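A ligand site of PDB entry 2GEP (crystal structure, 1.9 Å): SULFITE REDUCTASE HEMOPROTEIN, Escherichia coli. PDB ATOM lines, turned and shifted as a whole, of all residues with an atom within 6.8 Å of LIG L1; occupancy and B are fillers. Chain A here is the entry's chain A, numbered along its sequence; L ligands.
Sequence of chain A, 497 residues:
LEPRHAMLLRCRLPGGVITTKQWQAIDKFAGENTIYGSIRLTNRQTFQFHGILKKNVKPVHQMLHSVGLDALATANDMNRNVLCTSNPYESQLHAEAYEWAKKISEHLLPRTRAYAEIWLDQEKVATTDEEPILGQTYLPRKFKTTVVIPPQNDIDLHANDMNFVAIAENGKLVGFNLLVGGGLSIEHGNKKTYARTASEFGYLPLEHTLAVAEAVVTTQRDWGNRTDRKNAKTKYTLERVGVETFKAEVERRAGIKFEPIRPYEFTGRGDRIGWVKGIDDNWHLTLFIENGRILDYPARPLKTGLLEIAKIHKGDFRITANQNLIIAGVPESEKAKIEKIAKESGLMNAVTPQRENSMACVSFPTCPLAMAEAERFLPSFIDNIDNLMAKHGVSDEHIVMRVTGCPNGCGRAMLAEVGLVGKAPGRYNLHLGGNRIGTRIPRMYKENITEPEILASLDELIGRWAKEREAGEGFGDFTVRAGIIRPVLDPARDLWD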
ATOM      1  N   ALA A 360     -29.108 -32.304 -32.003  1.00  0.00           N
ATOM      2  CA  ALA A 360     -29.777 -31.269 -31.212  1.00  0.00           C
ATOM      3  C   ALA A 360     -28.853 -30.843 -30.080  1.00  0.00           C
ATOM      4  O   ALA A 360     -27.927 -31.571 -29.706  1.00  0.00           O
ATOM      5  CB  ALA A 360     -31.089 -31.786 -30.635  1.00  0.00           C
ATOM      6  N   CYS A 361     -29.064 -29.629 -29.584  1.00  0.00           N
ATOM      7  CA  CYS A 361     -28.285 -29.129 -28.461  1.00  0.00           C
ATOM      8  C   CYS A 361     -28.991 -29.593 -27.178  1.00  0.00           C
ATOM      9  O   CYS A 361     -30.067 -30.199 -27.220  1.00  0.00           O
ATOM     10  CB  CYS A 361     -28.187 -27.594 -28.483  1.00  0.00           C
ATOM     11  SG  CYS A 361     -29.769 -26.764 -28.125  1.00  0.00           S
ATOM     12  N   VAL A 362     -28.355 -29.322 -26.044  1.00  0.00           N
ATOM     13  CA  VAL A 362     -28.886 -29.708 -24.753  1.00  0.00           C
ATOM     14  C   VAL A 362     -30.246 -29.065 -24.449  1.00  0.00           C
ATOM     15  O   VAL A 362     -31.229 -29.766 -24.145  1.00  0.00           O
ATOM     16  CB  VAL A 362     -27.901 -29.346 -23.651  1.00  0.00           C
ATOM     17  CG1 VAL A 362     -28.476 -29.716 -22.302  1.00  0.00           C
ATOM     18  CG2 VAL A 362     -26.577 -30.063 -23.873  1.00  0.00           C
ATOM     19  N   SER A 363     -30.276 -27.738 -24.504  1.00  0.00           N
ATOM     20  CA  SER A 363     -31.486 -26.959 -24.223  1.00  0.00           C
ATOM     21  C   SER A 363     -32.035 -27.310 -22.815  1.00  0.00           C
ATOM     22  O   SER A 363     -31.241 -27.519 -21.888  1.00  0.00           O
ATOM     23  CB  SER A 363     -32.546 -27.210 -25.300  1.00  0.00           C
ATOM     24  OG  SER A 363     -33.623 -26.304 -25.131  1.00  0.00           O
ATOM     25  N   PHE A 364     -33.355 -27.359 -22.648  1.00  0.00           N
ATOM     26  CA  PHE A 364     -33.942 -27.663 -21.350  1.00  0.00           C
ATOM     27  C   PHE A 364     -33.554 -29.072 -21.004  1.00  0.00           C
ATOM     28  O   PHE A 364     -33.446 -29.897 -21.899  1.00  0.00           O
ATOM     29  CB  PHE A 364     -35.471 -27.572 -21.380  1.00  0.00           C
ATOM     30  CG  PHE A 364     -35.973 -26.213 -21.697  1.00  0.00           C
ATOM     31  CD1 PHE A 364     -35.800 -25.168 -20.786  1.00  0.00           C
ATOM     32  CD2 PHE A 364     -36.618 -25.963 -22.899  1.00  0.00           C
ATOM     33  CE1 PHE A 364     -36.267 -23.881 -21.081  1.00  0.00           C
ATOM     34  CE2 PHE A 364     -37.091 -24.681 -23.216  1.00  0.00           C
ATOM     35  CZ  PHE A 364     -36.918 -23.636 -22.304  1.00  0.00           C
ATOM     36  N   CYS A 367     -30.115 -25.733 -19.809  1.00  0.00           N
ATOM     37  CA  CYS A 367     -29.689 -24.474 -20.404  1.00  0.00           C
ATOM     38  C   CYS A 367     -30.528 -23.279 -19.991  1.00  0.00           C
ATOM     39  O   CYS A 367     -31.741 -23.266 -20.176  1.00  0.00           O
ATOM     40  CB  CYS A 367     -29.610 -24.575 -21.922  1.00  0.00           C
ATOM     41  SG  CYS A 367     -28.850 -23.072 -22.617  1.00  0.00           S
ATOM     42  N   PRO A 368     -29.876 -22.261 -19.431  1.00  0.00           N
ATOM     43  CA  PRO A 368     -30.578 -21.047 -18.997  1.00  0.00           C
ATOM     44  C   PRO A 368     -31.015 -20.130 -20.161  1.00  0.00           C
ATOM     45  O   PRO A 368     -31.850 -19.244 -19.975  1.00  0.00           O
ATOM     46  CB  PRO A 368     -29.558 -20.370 -18.084  1.00  0.00           C
ATOM     47  CG  PRO A 368     -28.253 -20.761 -18.714  1.00  0.00           C
ATOM     48  CD  PRO A 368     -28.450 -22.208 -19.034  1.00  0.00           C
ATOM     49  N   LEU A 369     -30.481 -20.368 -21.353  1.00  0.00           N
ATOM     50  CA  LEU A 369     -30.799 -19.543 -22.506  1.00  0.00           C
ATOM     51  C   LEU A 369     -31.797 -20.193 -23.441  1.00  0.00           C
ATOM     52  O   LEU A 369     -32.163 -19.619 -24.456  1.00  0.00           O
ATOM     53  CB  LEU A 369     -29.511 -19.219 -23.267  1.00  0.00           C
ATOM     54  CG  LEU A 369     -28.322 -18.728 -22.421  1.00  0.00           C
ATOM     55  CD1 LEU A 369     -27.084 -18.465 -23.284  1.00  0.00           C
ATOM     56  CD2 LEU A 369     -28.708 -17.463 -21.650  1.00  0.00           C
ATOM     57  N   ALA A 370     -32.258 -21.388 -23.065  1.00  0.00           N
ATOM     58  CA  ALA A 370     -33.199 -22.152 -23.891  1.00  0.00           C
ATOM     59  C   ALA A 370     -34.554 -21.504 -24.140  1.00  0.00           C
ATOM     60  O   ALA A 370     -35.207 -20.973 -23.234  1.00  0.00           O
ATOM     61  CB  ALA A 370     -33.399 -23.528 -23.288  1.00  0.00           C
ATOM     62  N   MET A 371     -34.994 -21.578 -25.389  1.00  0.00           N
ATOM     63  CA  MET A 371     -36.287 -21.026 -25.785  1.00  0.00           C
ATOM     64  C   MET A 371     -37.271 -22.167 -26.099  1.00  0.00           C
ATOM     65  O   MET A 371     -38.424 -22.116 -25.692  1.00  0.00           O
ATOM     66  CB  MET A 371     -36.119 -20.095 -26.986  1.00  0.00           C
ATOM     67  CG  MET A 371     -35.292 -18.841 -26.690  1.00  0.00           C
ATOM     68  SD  MET A 371     -34.991 -17.829 -28.183  1.00  0.00           S
ATOM     69  CE  MET A 371     -33.951 -16.501 -27.538  1.00  0.00           C
ATOM     70  N   ALA A 372     -36.777 -23.200 -26.771  1.00  0.00           N
ATOM     71  CA  ALA A 372     -37.589 -24.364 -27.132  1.00  0.00           C
ATOM     72  C   ALA A 372     -36.783 -25.617 -26.850  1.00  0.00           C
ATOM     73  O   ALA A 372     -35.552 -25.557 -26.784  1.00  0.00           O
ATOM     74  CB  ALA A 372     -37.939 -24.293 -28.607  1.00  0.00           C
ATOM     75  N   ALA A 374     -34.850 -29.117 -27.360  1.00  0.00           N
ATOM     76  CA  ALA A 374     -34.007 -29.573 -28.451  1.00  0.00           C
ATOM     77  C   ALA A 374     -33.679 -31.028 -28.196  1.00  0.00           C
ATOM     78  O   ALA A 374     -34.280 -31.920 -28.800  1.00  0.00           O
ATOM     79  CB  ALA A 374     -32.735 -28.733 -28.541  1.00  0.00           C
ATOM     80  N   VAL A 403     -31.541 -29.424 -34.628  1.00  0.00           N
ATOM     81  CA  VAL A 403     -32.430 -28.588 -33.866  1.00  0.00           C
ATOM     82  C   VAL A 403     -31.618 -27.892 -32.809  1.00  0.00           C
ATOM     83  O   VAL A 403     -30.881 -28.529 -32.045  1.00  0.00           O
ATOM     84  CB  VAL A 403     -33.517 -29.442 -33.169  1.00  0.00           C
ATOM     85  CG1 VAL A 403     -34.379 -28.581 -32.273  1.00  0.00           C
ATOM     86  CG2 VAL A 403     -34.381 -30.138 -34.216  1.00  0.00           C
ATOM     87  N   THR A 404     -31.691 -26.572 -32.787  1.00  0.00           N
ATOM     88  CA  THR A 404     -30.954 -25.799 -31.798  1.00  0.00           C
ATOM     89  C   THR A 404     -32.018 -25.103 -30.947  1.00  0.00           C
ATOM     90  O   THR A 404     -32.999 -24.580 -31.475  1.00  0.00           O
ATOM     91  CB  THR A 404     -29.931 -24.834 -32.502  1.00  0.00           C
ATOM     92  OG1 THR A 404     -28.970 -24.373 -31.558  1.00  0.00           O
ATOM     93  CG2 THR A 404     -30.618 -23.666 -33.188  1.00  0.00           C
ATOM     94  N   GLY A 405     -31.876 -25.197 -29.620  1.00  0.00           N
ATOM     95  CA  GLY A 405     -32.839 -24.627 -28.681  1.00  0.00           C
ATOM     96  C   GLY A 405     -33.034 -23.129 -28.661  1.00  0.00           C
ATOM     97  O   GLY A 405     -34.043 -22.645 -28.138  1.00  0.00           O
ATOM     98  N   CYS A 406     -32.077 -22.379 -29.195  1.00  0.00           N
ATOM     99  CA  CYS A 406     -32.156 -20.926 -29.263  1.00  0.00           C
ATOM    100  C   CYS A 406     -31.179 -20.518 -30.359  1.00  0.00           C
ATOM    101  O   CYS A 406     -30.362 -21.340 -30.789  1.00  0.00           O
ATOM    102  CB  CYS A 406     -31.828 -20.270 -27.901  1.00  0.00           C
ATOM    103  SG  CYS A 406     -30.061 -20.169 -27.453  1.00  0.00           S
ATOM    104  N   PRO A 407     -31.235 -19.266 -30.828  1.00  0.00           N
ATOM    105  CA  PRO A 407     -30.348 -18.795 -31.900  1.00  0.00           C
ATOM    106  C   PRO A 407     -28.815 -18.780 -31.655  1.00  0.00           C
ATOM    107  O   PRO A 407     -28.059 -18.609 -32.617  1.00  0.00           O
ATOM    108  CB  PRO A 407     -30.935 -17.425 -32.256  1.00  0.00           C
ATOM    109  CG  PRO A 407     -31.441 -16.938 -30.944  1.00  0.00           C
ATOM    110  CD  PRO A 407     -32.115 -18.177 -30.374  1.00  0.00           C
ATOM    111  N   ASN A 408     -28.370 -19.000 -30.423  1.00  0.00           N
ATOM    112  CA  ASN A 408     -26.931 -19.055 -30.117  1.00  0.00           C
ATOM    113  C   ASN A 408     -26.323 -20.147 -31.026  1.00  0.00           C
ATOM    114  O   ASN A 408     -25.143 -20.109 -31.358  1.00  0.00           O
ATOM    115  CB  ASN A 408     -26.696 -19.360 -28.639  1.00  0.00           C
ATOM    116  CG  ASN A 408     -26.879 -18.132 -27.756  1.00  0.00           C
ATOM    117  OD1 ASN A 408     -26.640 -17.010 -28.193  1.00  0.00           O
ATOM    118  ND2 ASN A 408     -27.308 -18.333 -26.530  1.00  0.00           N
ATOM    119  N   GLY A 409     -27.163 -21.094 -31.420  1.00  0.00           N
ATOM    120  CA  GLY A 409     -26.764 -22.111 -32.380  1.00  0.00           C
ATOM    121  C   GLY A 409     -25.889 -23.294 -32.056  1.00  0.00           C
ATOM    122  O   GLY A 409     -25.289 -23.865 -32.972  1.00  0.00           O
ATOM    123  N   CYS A 410     -25.873 -23.706 -30.796  1.00  0.00           N
ATOM    124  CA  CYS A 410     -25.071 -24.831 -30.361  1.00  0.00           C
ATOM    125  C   CYS A 410     -25.371 -26.138 -31.109  1.00  0.00           C
ATOM    126  O   CYS A 410     -24.465 -26.946 -31.326  1.00  0.00           O
ATOM    127  CB  CYS A 410     -25.277 -25.038 -28.860  1.00  0.00           C
ATOM    128  SG  CYS A 410     -25.058 -23.494 -27.910  1.00  0.00           S
ATOM    129  N   GLY A 411     -26.611 -26.341 -31.529  1.00  0.00           N
ATOM    130  CA  GLY A 411     -26.966 -27.557 -32.245  1.00  0.00           C
ATOM    131  C   GLY A 411     -26.488 -27.580 -33.684  1.00  0.00           C
ATOM    132  O   GLY A 411     -26.712 -28.564 -34.402  1.00  0.00           O
HETATM  133 FE1  LIG L   1     -29.202 -24.834 -27.059  1.00  0.00          FE
HETATM  134 FE2  LIG L   1     -28.746 -23.521 -24.788  1.00  0.00          FE
HETATM  135 FE3  LIG L   1     -29.347 -22.120 -26.963  1.00  0.00          FE
HETATM  136 FE4  LIG L   1     -27.018 -23.475 -26.833  1.00  0.00          FE
HETATM  137  S1  LIG L   1     -27.529 -21.723 -25.557  1.00  0.00           S
HETATM  138  S2  LIG L   1     -28.426 -23.309 -28.617  1.00  0.00           S
HETATM  139  S3  LIG L   1     -27.611 -25.363 -25.598  1.00  0.00           S
HETATM  140  S4  LIG L   1     -30.674 -23.675 -25.861  1.00  0.00           S
HETATM  141 FE1  LG2 L   2     -22.836 -23.556 -26.946  1.00  0.00          FE
HETATM  142  C1  LG2 L   2     -23.783 -21.049 -24.691  1.00  0.00           C
HETATM  143  C2  LG2 L   2     -24.108 -25.905 -24.850  1.00  0.00           C
HETATM  144  C3  LG2 L   2     -21.512 -25.997 -28.951  1.00  0.00           C
HETATM  145  C4  LG2 L   2     -22.702 -21.322 -29.414  1.00  0.00           C
HETATM  146  N1  LG2 L   2     -23.677 -23.482 -25.080  1.00  0.00           N
HETATM  147  C5  LG2 L   2     -23.850 -22.375 -24.228  1.00  0.00           C
HETATM  148  C6  LG2 L   2     -24.201 -22.838 -22.806  1.00  0.00           C
HETATM  149  C7  LG2 L   2     -22.855 -23.076 -22.049  1.00  0.00           C
HETATM  150  C8  LG2 L   2     -25.254 -21.976 -22.185  1.00  0.00           C
HETATM  151  C9  LG2 L   2     -24.809 -20.844 -21.291  1.00  0.00           C
HETATM  152  O1  LG2 L   2     -24.202 -19.869 -21.787  1.00  0.00           O
HETATM  153  O2  LG2 L   2     -25.060 -20.914 -20.073  1.00  0.00           O
HETATM  154  C10 LG2 L   2     -24.883 -24.069 -23.207  1.00  0.00           C
HETATM  155  C11 LG2 L   2     -24.903 -25.066 -22.095  1.00  0.00           C
HETATM  156  C12 LG2 L   2     -26.151 -25.905 -22.131  1.00  0.00           C
HETATM  157  C13 LG2 L   2     -26.130 -27.021 -21.108  1.00  0.00           C
HETATM  158  O3  LG2 L   2     -26.911 -26.944 -20.139  1.00  0.00           O
HETATM  159  O4  LG2 L   2     -25.343 -27.976 -21.252  1.00  0.00           O
HETATM  160  C14 LG2 L   2     -24.166 -24.585 -24.434  1.00  0.00           C
HETATM  161  N2  LG2 L   2     -22.729 -25.590 -26.861  1.00  0.00           N
HETATM  162  C15 LG2 L   2     -23.415 -26.381 -25.930  1.00  0.00           C
HETATM  163  C16 LG2 L   2     -23.123 -27.806 -26.330  1.00  0.00           C
HETATM  164  C17 LG2 L   2     -23.040 -28.779 -25.111  1.00  0.00           C
HETATM  165  C18 LG2 L   2     -24.320 -28.317 -27.321  1.00  0.00           C
HETATM  166  C19 LG2 L   2     -24.449 -29.805 -27.488  1.00  0.00           C
HETATM  167  O5  LG2 L   2     -25.554 -30.335 -27.321  1.00  0.00           O
HETATM  168  O6  LG2 L   2     -23.444 -30.475 -27.804  1.00  0.00           O
HETATM  169  C20 LG2 L   2     -21.752 -27.690 -27.019  1.00  0.00           C
HETATM  170  C21 LG2 L   2     -20.638 -27.658 -26.073  1.00  0.00           C
HETATM  171  C22 LG2 L   2     -19.389 -27.541 -26.924  1.00  0.00           C
HETATM  172  C23 LG2 L   2     -18.120 -27.750 -26.121  1.00  0.00           C
HETATM  173  O7  LG2 L   2     -17.989 -28.815 -25.493  1.00  0.00           O
HETATM  174  O8  LG2 L   2     -17.256 -26.860 -26.123  1.00  0.00           O
HETATM  175  C24 LG2 L   2     -21.979 -26.387 -27.717  1.00  0.00           C
HETATM  176  N3  LG2 L   2     -22.217 -23.633 -28.920  1.00  0.00           N
HETATM  177  C25 LG2 L   2     -21.663 -24.723 -29.486  1.00  0.00           C
HETATM  178  C26 LG2 L   2     -21.683 -24.419 -30.937  1.00  0.00           C
HETATM  179  C27 LG2 L   2     -21.285 -25.515 -31.901  1.00  0.00           C
HETATM  180  C28 LG2 L   2     -19.802 -25.757 -32.020  1.00  0.00           C
HETATM  181  O9  LG2 L   2     -19.016 -25.060 -31.348  1.00  0.00           O
HETATM  182  O10 LG2 L   2     -19.416 -26.664 -32.764  1.00  0.00           O
HETATM  183  C29 LG2 L   2     -21.999 -23.100 -31.156  1.00  0.00           C
HETATM  184  C30 LG2 L   2     -22.145 -22.529 -32.564  1.00  0.00           C
HETATM  185  C31 LG2 L   2     -20.884 -22.043 -33.248  1.00  0.00           C
HETATM  186  C32 LG2 L   2     -20.432 -20.708 -32.731  1.00  0.00           C
HETATM  187  O11 LG2 L   2     -19.845 -20.670 -31.638  1.00  0.00           O
HETATM  188  O12 LG2 L   2     -20.681 -19.686 -33.388  1.00  0.00           O
HETATM  189  C33 LG2 L   2     -22.327 -22.596 -29.801  1.00  0.00           C
HETATM  190  N4  LG2 L   2     -23.111 -21.546 -27.009  1.00  0.00           N
HETATM  191  C34 LG2 L   2     -23.004 -20.808 -28.197  1.00  0.00           C
HETATM  192  C35 LG2 L   2     -23.296 -19.417 -27.891  1.00  0.00           C
HETATM  193  C36 LG2 L   2     -23.388 -18.238 -28.852  1.00  0.00           C
HETATM  194  C37 LG2 L   2     -21.955 -17.777 -29.009  1.00  0.00           C
HETATM  195  C38 LG2 L   2     -21.821 -16.531 -29.851  1.00  0.00           C
HETATM  196  O13 LG2 L   2     -20.783 -16.372 -30.515  1.00  0.00           O
HETATM  197  O14 LG2 L   2     -22.742 -15.686 -29.836  1.00  0.00           O
HETATM  198  C39 LG2 L   2     -23.542 -19.385 -26.556  1.00  0.00           C
HETATM  199  C40 LG2 L   2     -23.951 -18.255 -25.700  1.00  0.00           C
HETATM  200  C41 LG2 L   2     -22.866 -17.241 -25.360  1.00  0.00           C
HETATM  201  O15 LG2 L   2     -21.675 -17.587 -25.413  1.00  0.00           O
HETATM  202  O16 LG2 L   2     -23.214 -16.094 -25.042  1.00  0.00           O
HETATM  203  C42 LG2 L   2     -23.479 -20.691 -25.994  1.00  0.00           C
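Leu 369 touches LIG L1 (CB to S1, 3.9 Å). CA of Ala 370 touches S4 of LIG L1, at 3.5 Å. Gly 405 touches LIG L1 (CA to S4, 3.7 Å). Hydrophobic or aromatic side chains within 4 Å of LIG L1: Leu 369 and Ala 370. Within 4 Å of LIG L1: Cys 361, Ser 363, Cys 367, Leu 369, Ala 370, Thr 404, Gly 405, Cys 406, Asn 408, Gly 409 and Cys 410. The nearest printed residue that does not touch LIG L1 is Val 362 (4.1 Å).
The side-chain sulfur (SG) of Cys 406 binds an iron atom (FE3) of LIG L1, 2.1 Å away. The side-chain sulfur of Cys 367 binds an iron atom (FE2) of LIG L1 (2.2 Å). N of Cys 410 sits close to S2 of LIG L1. FE4 of LIG L1 is bound by SG of Cys 410, at 2.2 Å. FE1 of LIG L1 is bound by SG of Cys 361 (2.3 Å). The side-chain hydroxyl of Thr 404 lies close to a sulfur (S2) of LIG L1, 3.2 Å away. ND2 of Asn 408 lies close to S1 of LIG L1. S3 of LIG L1 sits close to N of Ser 363, 3.7 Å away. A sulfur (S2) of LIG L1 lies close to the backbone NH (N) of Gly 409, 3.8 Å away. The backbone NH (N) of Cys 367 sits at hydrogen-bond distance from an oxygen (O3) of LG2 L2. The side-chain sulfur (SG) of Cys 410 binds an iron atom (FE1) of LG2 L2 (2.4 Å). N of Val 362 is in hydrogen-bond range of O5 of LG2 L2, at 3.2 Å.
OG1 of Thr 404 sits close to O of Cys 406, 3.4 Å away. ND2 of Asn 408 lies close to SG of Cys 406, at 3.4 Å. SG of Cys 406 lies close to O of Leu 369 (3.7 Å). N of Cys 410 lies within hydrogen-bond range of OG1 of Thr 404 (3.3 Å). SG of Cys 361 lies close to N of Gly 405 (3.0 Å). The backbone NH (N) of Ser 363 lies close to the side-chain sulfur (SG) of Cys 361 (3.8 Å). The backbone NH (N) of Gly 411 is in hydrogen-bond range of the side-chain hydroxyl (OG1) of Thr 404, at 3.1 Å. O of Gly 405 is in hydrogen-bond range of N of Ala 372.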
